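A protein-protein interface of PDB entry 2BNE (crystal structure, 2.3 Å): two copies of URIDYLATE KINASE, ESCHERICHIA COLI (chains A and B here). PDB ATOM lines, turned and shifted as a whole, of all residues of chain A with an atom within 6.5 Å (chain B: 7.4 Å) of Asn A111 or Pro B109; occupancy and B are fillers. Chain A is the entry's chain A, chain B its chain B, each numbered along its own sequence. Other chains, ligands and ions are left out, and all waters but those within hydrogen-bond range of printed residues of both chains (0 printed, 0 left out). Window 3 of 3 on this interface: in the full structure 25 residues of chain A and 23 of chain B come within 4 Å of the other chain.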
ATOM      1  N   ILE A 108     -18.528  38.983 -14.668  1.00  0.00           N
ATOM      2  CA  ILE A 108     -18.371  37.719 -13.967  1.00  0.00           C
ATOM      3  C   ILE A 108     -18.900  36.662 -14.919  1.00  0.00           C
ATOM      4  O   ILE A 108     -20.114  36.542 -15.105  1.00  0.00           O
ATOM      5  CB  ILE A 108     -19.216  37.673 -12.678  1.00  0.00           C
ATOM      6  CG1 ILE A 108     -18.557  38.512 -11.592  1.00  0.00           C
ATOM      7  CG2 ILE A 108     -19.404  36.233 -12.222  1.00  0.00           C
ATOM      8  CD1 ILE A 108     -19.327  38.516 -10.298  1.00  0.00           C
ATOM      9  N   PRO A 109     -17.999  35.877 -15.527  1.00  0.00           N
ATOM     10  CA  PRO A 109     -18.344  34.813 -16.479  1.00  0.00           C
ATOM     11  C   PRO A 109     -19.524  33.947 -16.048  1.00  0.00           C
ATOM     12  O   PRO A 109     -19.512  33.383 -14.958  1.00  0.00           O
ATOM     13  CB  PRO A 109     -17.052  34.007 -16.569  1.00  0.00           C
ATOM     14  CG  PRO A 109     -15.996  35.054 -16.375  1.00  0.00           C
ATOM     15  CD  PRO A 109     -16.554  35.869 -15.233  1.00  0.00           C
ATOM     16  N   LEU A 110     -20.536  33.845 -16.906  1.00  0.00           N
ATOM     17  CA  LEU A 110     -21.710  33.033 -16.612  1.00  0.00           C
ATOM     18  C   LEU A 110     -22.109  32.216 -17.839  1.00  0.00           C
ATOM     19  O   LEU A 110     -23.205  32.382 -18.383  1.00  0.00           O
ATOM     20  CB  LEU A 110     -22.882  33.918 -16.183  1.00  0.00           C
ATOM     21  CG  LEU A 110     -22.659  34.998 -15.116  1.00  0.00           C
ATOM     22  CD1 LEU A 110     -24.016  35.508 -14.667  1.00  0.00           C
ATOM     23  CD2 LEU A 110     -21.899  34.450 -13.917  1.00  0.00           C
ATOM     24  N   ASN A 111     -21.208  31.336 -18.267  1.00  0.00           N
ATOM     25  CA  ASN A 111     -21.415  30.471 -19.426  1.00  0.00           C
ATOM     26  C   ASN A 111     -22.877  30.092 -19.676  1.00  0.00           C
ATOM     27  O   ASN A 111     -23.621  29.783 -18.744  1.00  0.00           O
ATOM     28  CB  ASN A 111     -20.573  29.200 -19.267  1.00  0.00           C
ATOM     29  CG  ASN A 111     -20.661  28.275 -20.471  1.00  0.00           C
ATOM     30  OD1 ASN A 111     -21.742  27.814 -20.841  1.00  0.00           O
ATOM     31  ND2 ASN A 111     -19.516  27.997 -21.087  1.00  0.00           N
ATOM     32  N   GLY A 112     -23.274  30.115 -20.949  1.00  0.00           N
ATOM     33  CA  GLY A 112     -24.634  29.768 -21.326  1.00  0.00           C
ATOM     34  C   GLY A 112     -25.636  30.908 -21.221  1.00  0.00           C
ATOM     35  O   GLY A 112     -26.247  31.296 -22.224  1.00  0.00           O
ATOM     36  N   VAL A 113     -25.807  31.429 -20.005  1.00  0.00           N
ATOM     37  CA  VAL A 113     -26.729  32.531 -19.714  1.00  0.00           C
ATOM     38  C   VAL A 113     -26.485  33.751 -20.604  1.00  0.00           C
ATOM     39  O   VAL A 113     -27.393  34.246 -21.279  1.00  0.00           O
ATOM     40  CB  VAL A 113     -26.585  32.996 -18.250  1.00  0.00           C
ATOM     41  CG1 VAL A 113     -27.713  33.935 -17.893  1.00  0.00           C
ATOM     42  CG2 VAL A 113     -26.556  31.795 -17.322  1.00  0.00           C
ATOM     43  N   CYS A 114     -25.254  34.244 -20.574  1.00  0.00           N
ATOM     44  CA  CYS A 114     -24.866  35.400 -21.371  1.00  0.00           C
ATOM     45  C   CYS A 114     -23.386  35.271 -21.676  1.00  0.00           C
ATOM     46  O   CYS A 114     -22.787  34.224 -21.429  1.00  0.00           O
ATOM     47  CB  CYS A 114     -25.122  36.692 -20.596  1.00  0.00           C
ATOM     48  SG  CYS A 114     -24.240  36.780 -19.031  1.00  0.00           S
ATOM     49  N   LEU B  82     -30.542  31.466 -11.690  1.00  0.00           N
ATOM     50  CA  LEU B  82     -29.595  32.401 -11.089  1.00  0.00           C
ATOM     51  C   LEU B  82     -30.020  32.716  -9.664  1.00  0.00           C
ATOM     52  O   LEU B  82     -29.190  32.895  -8.774  1.00  0.00           O
ATOM     53  CB  LEU B  82     -29.524  33.706 -11.874  1.00  0.00           C
ATOM     54  CG  LEU B  82     -28.691  33.720 -13.149  1.00  0.00           C
ATOM     55  CD1 LEU B  82     -28.600  35.165 -13.655  1.00  0.00           C
ATOM     56  CD2 LEU B  82     -27.299  33.153 -12.872  1.00  0.00           C
ATOM     57  N   SER B 106     -22.442  25.025  -8.990  1.00  0.00           N
ATOM     58  CA  SER B 106     -23.536  25.522  -9.812  1.00  0.00           C
ATOM     59  C   SER B 106     -23.657  24.723 -11.114  1.00  0.00           C
ATOM     60  O   SER B 106     -22.651  24.436 -11.761  1.00  0.00           O
ATOM     61  CB  SER B 106     -23.293  27.013 -10.115  1.00  0.00           C
ATOM     62  OG  SER B 106     -24.300  27.562 -10.952  1.00  0.00           O
ATOM     63  N   ALA B 107     -24.884  24.363 -11.482  1.00  0.00           N
ATOM     64  CA  ALA B 107     -25.126  23.607 -12.712  1.00  0.00           C
ATOM     65  C   ALA B 107     -24.646  24.433 -13.886  1.00  0.00           C
ATOM     66  O   ALA B 107     -24.160  23.898 -14.873  1.00  0.00           O
ATOM     67  CB  ALA B 107     -26.603  23.286 -12.870  1.00  0.00           C
ATOM     68  N   ILE B 108     -24.784  25.745 -13.790  1.00  0.00           N
ATOM     69  CA  ILE B 108     -24.282  26.580 -14.858  1.00  0.00           C
ATOM     70  C   ILE B 108     -23.075  27.329 -14.312  1.00  0.00           C
ATOM     71  O   ILE B 108     -23.181  28.106 -13.365  1.00  0.00           O
ATOM     72  CB  ILE B 108     -25.363  27.538 -15.408  1.00  0.00           C
ATOM     73  CG1 ILE B 108     -25.866  28.485 -14.331  1.00  0.00           C
ATOM     74  CG2 ILE B 108     -26.526  26.712 -15.953  1.00  0.00           C
ATOM     75  CD1 ILE B 108     -27.065  29.290 -14.782  1.00  0.00           C
ATOM     76  N   PRO B 109     -21.897  27.079 -14.906  1.00  0.00           N
ATOM     77  CA  PRO B 109     -20.627  27.697 -14.513  1.00  0.00           C
ATOM     78  C   PRO B 109     -20.699  29.202 -14.329  1.00  0.00           C
ATOM     79  O   PRO B 109     -21.141  29.934 -15.212  1.00  0.00           O
ATOM     80  CB  PRO B 109     -19.676  27.274 -15.633  1.00  0.00           C
ATOM     81  CG  PRO B 109     -20.586  27.118 -16.816  1.00  0.00           C
ATOM     82  CD  PRO B 109     -21.763  26.405 -16.210  1.00  0.00           C
ATOM     83  N   LEU B 110     -20.261  29.639 -13.155  1.00  0.00           N
ATOM     84  CA  LEU B 110     -20.244  31.035 -12.771  1.00  0.00           C
ATOM     85  C   LEU B 110     -18.899  31.235 -12.088  1.00  0.00           C
ATOM     86  O   LEU B 110     -18.767  31.990 -11.124  1.00  0.00           O
ATOM     87  CB  LEU B 110     -21.385  31.311 -11.793  1.00  0.00           C
ATOM     88  CG  LEU B 110     -22.735  30.752 -12.256  1.00  0.00           C
ATOM     89  CD1 LEU B 110     -23.739  30.851 -11.135  1.00  0.00           C
ATOM     90  CD2 LEU B 110     -23.219  31.501 -13.489  1.00  0.00           C
ATOM     91  N   ASN B 111     -17.908  30.521 -12.608  1.00  0.00           N
ATOM     92  CA  ASN B 111     -16.537  30.545 -12.110  1.00  0.00           C
ATOM     93  C   ASN B 111     -16.155  31.866 -11.446  1.00  0.00           C
ATOM     94  O   ASN B 111     -16.481  32.943 -11.947  1.00  0.00           O
ATOM     95  CB  ASN B 111     -15.586  30.240 -13.270  1.00  0.00           C
ATOM     96  CG  ASN B 111     -16.072  29.081 -14.124  1.00  0.00           C
ATOM     97  OD1 ASN B 111     -16.236  27.961 -13.635  1.00  0.00           O
ATOM     98  ND2 ASN B 111     -16.313  29.347 -15.407  1.00  0.00           N
ATOM     99  N   GLY B 112     -15.456  31.764 -10.316  1.00  0.00           N
ATOM    100  CA  GLY B 112     -15.032  32.941  -9.575  1.00  0.00           C
ATOM    101  C   GLY B 112     -15.848  33.121  -8.306  1.00  0.00           C
ATOM    102  O   GLY B 112     -15.302  33.281  -7.211  1.00  0.00           O
ATOM    103  N   CYS B 114     -18.331  30.819  -7.506  1.00  0.00           N
ATOM    104  CA  CYS B 114     -18.545  29.473  -6.981  1.00  0.00           C
ATOM    105  C   CYS B 114     -18.068  28.422  -7.958  1.00  0.00           C
ATOM    106  O   CYS B 114     -17.867  28.693  -9.143  1.00  0.00           O
ATOM    107  CB  CYS B 114     -20.025  29.216  -6.650  1.00  0.00           C
ATOM    108  SG  CYS B 114     -21.154  29.084  -8.060  1.00  0.00           S
ATOM    109  N   ASP B 115     -17.892  27.217  -7.438  1.00  0.00           N
ATOM    110  CA  ASP B 115     -17.445  26.083  -8.222  1.00  0.00           C
ATOM    111  C   ASP B 115     -18.491  25.658  -9.230  1.00  0.00           C
ATOM    112  O   ASP B 115     -19.682  25.894  -9.059  1.00  0.00           O
ATOM    113  CB  ASP B 115     -17.156  24.892  -7.302  1.00  0.00           C
ATOM    114  CG  ASP B 115     -15.769  24.942  -6.685  1.00  0.00           C
ATOM    115  OD1 ASP B 115     -15.198  26.053  -6.585  1.00  0.00           O
ATOM    116  OD2 ASP B 115     -15.257  23.865  -6.288  1.00  0.00           O
ATOM    117  N   SER B 116     -18.025  25.011 -10.284  1.00  0.00           N
ATOM    118  CA  SER B 116     -18.909  24.489 -11.303  1.00  0.00           C
ATOM    119  C   SER B 116     -19.250  23.085 -10.789  1.00  0.00           C
ATOM    120  O   SER B 116     -18.356  22.361 -10.340  1.00  0.00           O
ATOM    121  CB  SER B 116     -18.161  24.418 -12.632  1.00  0.00           C
ATOM    122  OG  SER B 116     -19.035  24.064 -13.683  1.00  0.00           O
ATOM    123  N   TYR B 117     -20.526  22.707 -10.822  1.00  0.00           N
ATOM    124  CA  TYR B 117     -20.921  21.386 -10.334  1.00  0.00           C
ATOM    125  C   TYR B 117     -20.119  20.287 -10.991  1.00  0.00           C
ATOM    126  O   TYR B 117     -19.974  20.266 -12.209  1.00  0.00           O
ATOM    127  CB  TYR B 117     -22.401  21.099 -10.591  1.00  0.00           C
ATOM    128  CG  TYR B 117     -22.762  19.647 -10.328  1.00  0.00           C
ATOM    129  CD1 TYR B 117     -22.690  19.115  -9.044  1.00  0.00           C
ATOM    130  CD2 TYR B 117     -23.141  18.796 -11.367  1.00  0.00           C
ATOM    131  CE1 TYR B 117     -22.983  17.775  -8.796  1.00  0.00           C
ATOM    132  CE2 TYR B 117     -23.440  17.450 -11.129  1.00  0.00           C
ATOM    133  CZ  TYR B 117     -23.358  16.951  -9.842  1.00  0.00           C
ATOM    134  OH  TYR B 117     -23.661  15.632  -9.585  1.00  0.00           O
ATOM    135  N   ALA B 136     -28.565  26.267  -9.269  1.00  0.00           N
ATOM    136  CA  ALA B 136     -28.948  26.319 -10.681  1.00  0.00           C
ATOM    137  C   ALA B 136     -29.656  25.017 -11.040  1.00  0.00           C
ATOM    138  O   ALA B 136     -29.754  24.642 -12.216  1.00  0.00           O
ATOM    139  CB  ALA B 136     -27.737  26.510 -11.561  1.00  0.00           C
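Of the printed residues of chain B, Pro A109 touches Pro B109 and Leu B110. Of the printed residues of chain B, Leu A110 touches Pro B109 (3.4 Å) and Leu B110 (3.3 Å). Asn A111 touches just one residue of chain B: Pro B109 (3.2 Å). Of the printed residues of chain B, Val A113 touches Ile B108. Of the printed residues of chain A, Pro B109 touches Pro A109, Leu A110 and Asn A111. Of the printed residues of chain A, Leu B110 touches Pro A109 (3.3 Å) and Leu A110 (3.3 Å). The nearest residue of chain B that does not touch Asn A111 is Ile B108 (4.4 Å). The nearest residue of chain A that does not touch Pro B109 is Gly A112 (5.8 Å).
The side-chain hydroxyl of Ser B106 lies within hydrogen-bond range of the backbone carbonyl oxygen of Ile B108 (2.7 Å).
Of the 7 printed residues of chain A, 4 touch a printed residue of chain B. Of the 13 printed residues of chain B, 3 touch a printed residue of chain A.
Among the printed residues, merely in contact across the chains: Leu A110 with Leu B110 (3.3 Å), Pro A109 with Leu B110 (3.3 Å), Leu A110 with Pro B109 (3.4 Å), Val A113 with Ile B108 (3.6 Å) and Pro A109 with Pro B109 (3.8 Å).
Pro A109 touches its own counterpart, Pro B109. Pro A109 touches Leu B110, and with the chains exchanged Leu A110 touches Pro B109. Leu A110 touches its own counterpart, Leu B110. Asn A111 touches Pro B109, but with the chains exchanged Pro A109 does not touch Asn B111 (4.04 Å). Positions printed for both chains: 108, 109, 110, 111, 112 and 114. Of the 6 pairs that touch across the chains among the printed residues, 4 have their exchanged pair printed and touching as well.
The backbone NH (N) of Asn A111 sits at hydrogen-bond distance from the backbone carbonyl oxygen (O) of Pro B109, at 3.4 Å.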
